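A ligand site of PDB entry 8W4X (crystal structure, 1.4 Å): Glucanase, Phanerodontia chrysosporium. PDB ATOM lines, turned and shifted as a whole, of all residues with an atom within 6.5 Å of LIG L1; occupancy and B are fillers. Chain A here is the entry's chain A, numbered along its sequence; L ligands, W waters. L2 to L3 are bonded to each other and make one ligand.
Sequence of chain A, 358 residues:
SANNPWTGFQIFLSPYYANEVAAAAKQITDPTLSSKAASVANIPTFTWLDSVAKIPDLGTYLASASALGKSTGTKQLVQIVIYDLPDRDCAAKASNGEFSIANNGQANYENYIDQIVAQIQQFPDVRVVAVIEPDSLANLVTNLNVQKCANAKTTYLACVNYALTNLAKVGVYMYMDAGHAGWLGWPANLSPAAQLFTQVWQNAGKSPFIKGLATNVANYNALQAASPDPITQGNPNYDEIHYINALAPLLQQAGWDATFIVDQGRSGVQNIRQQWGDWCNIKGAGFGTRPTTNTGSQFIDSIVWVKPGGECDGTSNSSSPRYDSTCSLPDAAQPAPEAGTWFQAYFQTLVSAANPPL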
ATOM      1  N   TRP A  48      12.284  10.719   0.090  1.00  0.00           N
ATOM      2  CA  TRP A  48      13.605  10.850  -0.484  1.00  0.00           C
ATOM      3  C   TRP A  48      14.225  12.177  -0.088  1.00  0.00           C
ATOM      4  O   TRP A  48      13.639  13.248  -0.297  1.00  0.00           O
ATOM      5  CB  TRP A  48      13.550  10.763  -2.000  1.00  0.00           C
ATOM      6  CG  TRP A  48      13.201   9.400  -2.511  1.00  0.00           C
ATOM      7  CD1 TRP A  48      12.078   8.660  -2.195  1.00  0.00           C
ATOM      8  CD2 TRP A  48      13.951   8.622  -3.438  1.00  0.00           C
ATOM      9  NE1 TRP A  48      12.106   7.469  -2.877  1.00  0.00           N
ATOM     10  CE2 TRP A  48      13.240   7.410  -3.643  1.00  0.00           C
ATOM     11  CE3 TRP A  48      15.143   8.819  -4.121  1.00  0.00           C
ATOM     12  CZ2 TRP A  48      13.686   6.434  -4.507  1.00  0.00           C
ATOM     13  CZ3 TRP A  48      15.591   7.848  -4.972  1.00  0.00           C
ATOM     14  CH2 TRP A  48      14.871   6.657  -5.183  1.00  0.00           C
ATOM     15  N   LEU A  49      15.449  12.125   0.414  1.00  0.00           N
ATOM     16  CA  LEU A  49      16.241  13.325   0.730  1.00  0.00           C
ATOM     17  C   LEU A  49      17.147  13.552  -0.480  1.00  0.00           C
ATOM     18  O   LEU A  49      18.341  13.268  -0.485  1.00  0.00           O
ATOM     19  CB  LEU A  49      17.026  13.187   2.030  1.00  0.00           C
ATOM     20  CG  LEU A  49      16.130  12.866   3.238  1.00  0.00           C
ATOM     21  CD1 LEU A  49      16.971  12.625   4.459  1.00  0.00           C
ATOM     22  CD2 LEU A  49      15.164  13.980   3.440  1.00  0.00           C
ATOM     23  N   ASP A  50      16.542  14.050  -1.564  1.00  0.00           N
ATOM     24  CA  ASP A  50      17.216  14.213  -2.837  1.00  0.00           C
ATOM     25  C   ASP A  50      17.884  15.566  -2.987  1.00  0.00           C
ATOM     26  O   ASP A  50      18.459  15.815  -4.047  1.00  0.00           O
ATOM     27  CB  ASP A  50      16.206  13.971  -3.975  1.00  0.00           C
ATOM     28  CG  ASP A  50      15.080  14.970  -4.003  1.00  0.00           C
ATOM     29  OD1 ASP A  50      14.528  15.297  -2.938  1.00  0.00           O
ATOM     30  OD2 ASP A  50      14.716  15.392  -5.123  1.00  0.00           O
ATOM     31  N   LYS A  54      15.936  19.562   1.687  1.00  0.00           N
ATOM     32  CA  LYS A  54      14.931  18.760   2.354  1.00  0.00           C
ATOM     33  C   LYS A  54      15.317  18.356   3.751  1.00  0.00           C
ATOM     34  O   LYS A  54      14.498  17.764   4.446  1.00  0.00           O
ATOM     35  CB  LYS A  54      14.628  17.543   1.490  1.00  0.00           C
ATOM     36  CG  LYS A  54      13.985  18.001   0.174  1.00  0.00           C
ATOM     37  CD  LYS A  54      13.199  16.933  -0.402  1.00  0.00           C
ATOM     38  CE  LYS A  54      12.451  17.399  -1.667  1.00  0.00           C
ATOM     39  NZ  LYS A  54      12.026  16.140  -2.369  1.00  0.00           N
ATOM     40  N   TYR A  83      19.908  10.201  -1.122  1.00  0.00           N
ATOM     41  CA  TYR A  83      20.061  10.215  -2.592  1.00  0.00           C
ATOM     42  C   TYR A  83      20.607  11.577  -3.025  1.00  0.00           C
ATOM     43  O   TYR A  83      19.889  12.419  -3.593  1.00  0.00           O
ATOM     44  CB  TYR A  83      18.735   9.934  -3.285  1.00  0.00           C
ATOM     45  CG  TYR A  83      18.796   9.770  -4.794  1.00  0.00           C
ATOM     46  CD1 TYR A  83      19.566   8.764  -5.365  1.00  0.00           C
ATOM     47  CD2 TYR A  83      18.056  10.574  -5.624  1.00  0.00           C
ATOM     48  CE1 TYR A  83      19.609   8.566  -6.739  1.00  0.00           C
ATOM     49  CE2 TYR A  83      18.077  10.399  -6.986  1.00  0.00           C
ATOM     50  CZ  TYR A  83      18.842   9.387  -7.538  1.00  0.00           C
ATOM     51  OH  TYR A  83      18.884   9.259  -8.926  1.00  0.00           O
ATOM     52  N   ARG A  88      25.675  12.405  -9.278  1.00  0.00           N
ATOM     53  CA  ARG A  88      24.617  11.409  -9.113  1.00  0.00           C
ATOM     54  C   ARG A  88      24.149  10.897 -10.462  1.00  0.00           C
ATOM     55  O   ARG A  88      24.195  11.602 -11.470  1.00  0.00           O
ATOM     56  CB  ARG A  88      23.453  12.107  -8.381  1.00  0.00           C
ATOM     57  CG  ARG A  88      22.396  11.185  -7.769  1.00  0.00           C
ATOM     58  CD  ARG A  88      21.394  11.955  -6.947  1.00  0.00           C
ATOM     59  NE  ARG A  88      20.517  12.773  -7.752  1.00  0.00           N
ATOM     60  CZ  ARG A  88      19.675  13.679  -7.279  1.00  0.00           C
ATOM     61  NH1 ARG A  88      19.548  13.888  -5.986  1.00  0.00           N
ATOM     62  NH2 ARG A  88      18.928  14.382  -8.127  1.00  0.00           N
ATOM     63  N   ALA A  94      18.722  11.826 -16.423  1.00  0.00           N
ATOM     64  CA  ALA A  94      17.469  12.439 -15.980  1.00  0.00           C
ATOM     65  C   ALA A  94      17.485  12.895 -14.532  1.00  0.00           C
ATOM     66  O   ALA A  94      16.716  13.777 -14.144  1.00  0.00           O
ATOM     67  CB  ALA A  94      16.338  11.464 -16.167  1.00  0.00           C
ATOM     68  N   SER A  95      18.356  12.288 -13.681  1.00  0.00           N
ATOM     69  CA  SER A  95      18.343  12.571 -12.255  1.00  0.00           C
ATOM     70  C   SER A  95      19.681  13.107 -11.766  1.00  0.00           C
ATOM     71  O   SER A  95      20.048  12.962 -10.590  1.00  0.00           O
ATOM     72  CB  SER A  95      17.920  11.354 -11.434  1.00  0.00           C
ATOM     73  OG  SER A  95      16.513  11.113 -11.507  1.00  0.00           O
ATOM     74  N   ASN A  96      20.429  13.775 -12.649  1.00  0.00           N
ATOM     75  CA  ASN A  96      21.584  14.537 -12.206  1.00  0.00           C
ATOM     76  C   ASN A  96      21.181  15.474 -11.077  1.00  0.00           C
ATOM     77  O   ASN A  96      20.083  16.028 -11.081  1.00  0.00           O
ATOM     78  CB  ASN A  96      22.148  15.318 -13.400  1.00  0.00           C
ATOM     79  CG  ASN A  96      23.370  16.139 -13.020  1.00  0.00           C
ATOM     80  OD1 ASN A  96      24.244  15.652 -12.306  1.00  0.00           O
ATOM     81  ND2 ASN A  96      23.417  17.401 -13.472  1.00  0.00           N
ATOM     82  N   ALA A 218      12.744   1.810  -7.575  1.00  0.00           N
ATOM     83  CA  ALA A 218      12.319   2.571  -8.746  1.00  0.00           C
ATOM     84  C   ALA A 218      12.213   1.725 -10.003  1.00  0.00           C
ATOM     85  O   ALA A 218      12.126   2.278 -11.107  1.00  0.00           O
ATOM     86  CB  ALA A 218      13.225   3.803  -8.999  1.00  0.00           C
ATOM     87  N   VAL A 306       9.448   2.034  -2.184  1.00  0.00           N
ATOM     88  CA  VAL A 306      10.539   2.980  -2.046  1.00  0.00           C
ATOM     89  C   VAL A 306      10.342   4.159  -2.973  1.00  0.00           C
ATOM     90  O   VAL A 306      10.245   5.300  -2.513  1.00  0.00           O
ATOM     91  CB  VAL A 306      11.920   2.333  -2.191  1.00  0.00           C
ATOM     92  CG1 VAL A 306      13.006   3.377  -1.890  1.00  0.00           C
ATOM     93  CG2 VAL A 306      12.067   1.134  -1.261  1.00  0.00           C
ATOM     94  N   LYS A 307      10.308   3.924  -4.290  1.00  0.00           N
ATOM     95  CA  LYS A 307       9.957   4.959  -5.240  1.00  0.00           C
ATOM     96  C   LYS A 307       8.482   5.319  -5.111  1.00  0.00           C
ATOM     97  O   LYS A 307       7.643   4.426  -5.249  1.00  0.00           O
ATOM     98  CB  LYS A 307      10.249   4.464  -6.647  1.00  0.00           C
ATOM     99  CG  LYS A 307       9.731   5.323  -7.791  1.00  0.00           C
ATOM    100  CD  LYS A 307      10.522   6.625  -7.947  1.00  0.00           C
ATOM    101  CE  LYS A 307       9.867   7.501  -9.013  1.00  0.00           C
ATOM    102  NZ  LYS A 307      10.691   8.695  -9.318  1.00  0.00           N
ATOM    103  N   PRO A 308       8.103   6.564  -4.828  1.00  0.00           N
ATOM    104  CA  PRO A 308       6.685   6.886  -4.665  1.00  0.00           C
ATOM    105  C   PRO A 308       6.003   7.029  -6.013  1.00  0.00           C
ATOM    106  O   PRO A 308       6.339   7.899  -6.811  1.00  0.00           O
ATOM    107  CB  PRO A 308       6.709   8.218  -3.889  1.00  0.00           C
ATOM    108  CG  PRO A 308       8.146   8.396  -3.390  1.00  0.00           C
ATOM    109  CD  PRO A 308       8.970   7.698  -4.469  1.00  0.00           C
ATOM    110  N   GLU A 311       5.580  10.228  -8.727  1.00  0.00           N
ATOM    111  CA  GLU A 311       6.717  11.107  -8.916  1.00  0.00           C
ATOM    112  C   GLU A 311       7.521  10.640 -10.118  1.00  0.00           C
ATOM    113  O   GLU A 311       7.850   9.461 -10.246  1.00  0.00           O
ATOM    114  CB  GLU A 311       7.575  11.113  -7.645  1.00  0.00           C
ATOM    115  CG  GLU A 311       6.829  11.702  -6.459  1.00  0.00           C
ATOM    116  CD  GLU A 311       7.617  11.749  -5.183  1.00  0.00           C
ATOM    117  OE1 GLU A 311       8.844  11.406  -5.185  1.00  0.00           O
ATOM    118  OE2 GLU A 311       6.995  12.113  -4.157  1.00  0.00           O
ATOM    119  N   CYS A 312       7.773  11.554 -11.041  1.00  0.00           N
ATOM    120  CA  CYS A 312       8.297  11.199 -12.354  1.00  0.00           C
ATOM    121  C   CYS A 312       9.731  10.667 -12.285  1.00  0.00           C
ATOM    122  O   CYS A 312      10.509  11.010 -11.387  1.00  0.00           O
ATOM    123  CB  CYS A 312       8.226  12.464 -13.227  1.00  0.00           C
ATOM    124  SG  CYS A 312       8.656  12.221 -14.957  1.00  0.00           S
ATOM    125  N   ASP A 313      10.111   9.852 -13.279  1.00  0.00           N
ATOM    126  CA  ASP A 313      11.455   9.332 -13.398  1.00  0.00           C
ATOM    127  C   ASP A 313      12.368  10.178 -14.267  1.00  0.00           C
ATOM    128  O   ASP A 313      13.583   9.982 -14.243  1.00  0.00           O
ATOM    129  CB  ASP A 313      11.464   7.920 -14.007  1.00  0.00           C
ATOM    130  CG  ASP A 313      10.756   6.889 -13.193  1.00  0.00           C
ATOM    131  OD1 ASP A 313      10.955   6.896 -11.972  1.00  0.00           O
ATOM    132  OD2 ASP A 313      10.036   6.063 -13.783  1.00  0.00           O
ATOM    133  N   GLY A 314      11.817  11.091 -15.043  1.00  0.00           N
ATOM    134  CA  GLY A 314      12.609  11.857 -15.984  1.00  0.00           C
ATOM    135  C   GLY A 314      11.739  12.462 -17.069  1.00  0.00           C
ATOM    136  O   GLY A 314      10.689  11.923 -17.394  1.00  0.00           O
ATOM    137  N   ARG A 322      18.372  17.707 -18.640  1.00  0.00           N
ATOM    138  CA  ARG A 322      18.247  16.379 -18.034  1.00  0.00           C
ATOM    139  C   ARG A 322      17.464  15.432 -18.928  1.00  0.00           C
ATOM    140  O   ARG A 322      16.939  14.431 -18.455  1.00  0.00           O
ATOM    141  CB  ARG A 322      17.606  16.510 -16.640  1.00  0.00           C
ATOM    142  CG  ARG A 322      18.458  17.382 -15.707  1.00  0.00           C
ATOM    143  CD  ARG A 322      18.304  17.005 -14.240  1.00  0.00           C
ATOM    144  NE  ARG A 322      16.900  17.060 -13.859  1.00  0.00           N
ATOM    145  CZ  ARG A 322      16.409  16.620 -12.714  1.00  0.00           C
ATOM    146  NH1 ARG A 322      17.188  16.136 -11.777  1.00  0.00           N
ATOM    147  NH2 ARG A 322      15.099  16.656 -12.518  1.00  0.00           N
ATOM    148  N   ALA A 339      12.232  14.785 -13.589  1.00  0.00           N
ATOM    149  CA  ALA A 339      12.330  13.756 -12.539  1.00  0.00           C
ATOM    150  C   ALA A 339      12.034  14.350 -11.181  1.00  0.00           C
ATOM    151  O   ALA A 339      12.503  15.445 -10.843  1.00  0.00           O
ATOM    152  CB  ALA A 339      13.714  13.145 -12.535  1.00  0.00           C
ATOM    153  N   GLY A 340      11.266  13.609 -10.365  1.00  0.00           N
ATOM    154  CA  GLY A 340      10.939  14.008  -9.036  1.00  0.00           C
ATOM    155  C   GLY A 340       9.680  14.855  -8.924  1.00  0.00           C
ATOM    156  O   GLY A 340       9.144  14.993  -7.823  1.00  0.00           O
ATOM    157  N   THR A 341       9.172  15.391 -10.005  1.00  0.00           N
ATOM    158  CA  THR A 341       7.945  16.170  -9.958  1.00  0.00           C
ATOM    159  C   THR A 341       6.731  15.301 -10.210  1.00  0.00           C
ATOM    160  O   THR A 341       6.829  14.176 -10.708  1.00  0.00           O
ATOM    161  CB  THR A 341       8.004  17.332 -10.934  1.00  0.00           C
ATOM    162  OG1 THR A 341       7.979  16.856 -12.262  1.00  0.00           O
ATOM    163  CG2 THR A 341       9.262  18.139 -10.720  1.00  0.00           C
HETATM  164  C1  LIG L   1      14.289  11.755  -8.671  1.00  0.00           C
HETATM  165  C2  LIG L   1      14.226  12.322  -7.275  1.00  0.00           C
HETATM  166  C3  LIG L   1      13.035  11.826  -6.515  1.00  0.00           C
HETATM  167  C4  LIG L   1      12.962  10.360  -6.519  1.00  0.00           C
HETATM  168  C5  LIG L   1      11.716   9.805  -5.895  1.00  0.00           C
HETATM  169  C6  LIG L   1      14.239  10.219  -8.636  1.00  0.00           C
HETATM  170  O1  LIG L   1      14.170   9.635  -9.823  1.00  0.00           O
HETATM  171  O2  LIG L   1      15.524  12.114  -9.266  1.00  0.00           O
HETATM  172  O3  LIG L   1      14.185  13.771  -7.355  1.00  0.00           O
HETATM  173  O4  LIG L   1      13.228  12.234  -5.132  1.00  0.00           O
HETATM  174  O5  LIG L   1      12.997   9.844  -7.876  1.00  0.00           O
HETATM  175  O6  LIG L   1      10.567  10.087  -6.720  1.00  0.00           O
HETATM  176  C1  LG2 L   2      20.196  -1.820 -16.982  1.00  0.00           C
HETATM  177  C2  LG2 L   2      19.110  -1.753 -15.925  1.00  0.00           C
HETATM  178  C3  LG2 L   2      18.628  -0.324 -15.681  1.00  0.00           C
HETATM  179  C4  LG2 L   2      19.782   0.587 -15.378  1.00  0.00           C
HETATM  180  C5  LG2 L   2      20.858   0.466 -16.473  1.00  0.00           C
HETATM  181  C6  LG2 L   2      22.017   1.239 -15.973  1.00  0.00           C
HETATM  182  O1  LG2 L   2      19.692  -1.494 -18.259  1.00  0.00           O
HETATM  183  O2  LG2 L   2      17.968  -2.558 -16.260  1.00  0.00           O
HETATM  184  O3  LG2 L   2      17.694  -0.402 -14.542  1.00  0.00           O
HETATM  185  O4  LG2 L   2      19.347   1.952 -15.438  1.00  0.00           O
HETATM  186  O5  LG2 L   2      21.221  -0.882 -16.639  1.00  0.00           O
HETATM  187  O6  LG2 L   2      22.944   1.372 -17.173  1.00  0.00           O
HETATM  188  C1  LG3 L   3      19.063   4.117 -14.497  1.00  0.00           C
HETATM  189  C2  LG3 L   3      18.699   4.835 -13.238  1.00  0.00           C
HETATM  190  C3  LG3 L   3      17.396   4.263 -12.664  1.00  0.00           C
HETATM  191  C4  LG3 L   3      17.512   2.772 -12.481  1.00  0.00           C
HETATM  192  C5  LG3 L   3      16.208   2.148 -12.081  1.00  0.00           C
HETATM  193  C6  LG3 L   3      19.132   2.636 -14.237  1.00  0.00           C
HETATM  194  O1  LG3 L   3      20.341   4.554 -14.954  1.00  0.00           O
HETATM  195  O2  LG3 L   3      18.460   6.261 -13.500  1.00  0.00           O
HETATM  196  O3  LG3 L   3      17.048   4.945 -11.464  1.00  0.00           O
HETATM  197  O4  LG3 L   3      17.852   2.197 -13.770  1.00  0.00           O
HETATM  198  O5  LG3 L   3      16.334   0.740 -11.958  1.00  0.00           O
HETATM  199  O   HOH W   1      16.470   8.039  -9.923  1.00  0.00           O
HETATM  200  O   HOH W   2      15.873  14.866  -9.641  1.00  0.00           O
HETATM  201  O   HOH W   3      10.751  12.825  -3.924  1.00  0.00           O
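N of Gly 340 is in hydrogen-bond range of O of Cys 312 (2.9 Å).
O of Ala 339 lies within hydrogen-bond range of NH2 of Arg 322, at 3.3 Å.
The side-chain amino group (NZ) of Lys 307 lies within salt-bridge range of the side-chain carboxylate (OD1) of Asp 313 (3.2 Å).
The backbone carbonyl oxygen (O) of Tyr 83 is in hydrogen-bond range of the guanidinium group (NH1) of Arg 88 (2.8 Å).
NZ of Lys 307 lies within hydrogen-bond range of O of Cys 312 (3.1 Å).
NZ of Lys 307 sits close to O of Glu 311, 3.1 Å away.
O of Val 306 sits at hydrogen-bond distance from NE1 of Trp 48.
NE of Arg 88 sits at hydrogen-bond distance from O of Ser 95 (2.9 Å).
Water W2 lies within hydrogen-bond range of O2 of LIG L1 (2.8 Å), NH1 of Arg 322 (2.8 Å) and NH2 of Arg 88 (3.4 Å).
Water W1 lies within hydrogen-bond range of an oxygen (O1) of LIG L1, the side-chain hydroxyl of Tyr 83 and the side-chain hydroxyl of Ser 95.
Water W3 lies within hydrogen-bond range of OE1 of Glu 311 (2.7 Å) and O4 of LIG L1 (2.8 Å).
An oxygen (O2) of LIG L1 is in hydrogen-bond range of the side-chain hydroxyl (OG) of Ser 95, at 2.6 Å.
OE1 of Glu 311 is in hydrogen-bond range of O6 of LIG L1.
O6 of LIG L1 is in hydrogen-bond range of NZ of Lys 307, at 3.0 Å.
OD2 of Asp 50 is in hydrogen-bond range of O3 of LIG L1.
Merely in contact with LIG L1: Trp 48 (3.5 Å), Pro 308 (3.7 Å), Gly 340 (3.7 Å), Tyr 83 (3.8 Å) and Ala 339 (3.9 Å).
Hydrophobic or aromatic side chains that line LIG L1: Trp 48, Tyr 83, Pro 308 and Ala 339.
Nine residues have an atom within 4 Å of LIG L1: Trp 48, Asp 50, Tyr 83, Ser 95, Lys 307, Pro 308, Glu 311, Ala 339 and Gly 340.
The nearest printed residue that does not touch LIG L1 is Cys 312 (4.2 Å).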
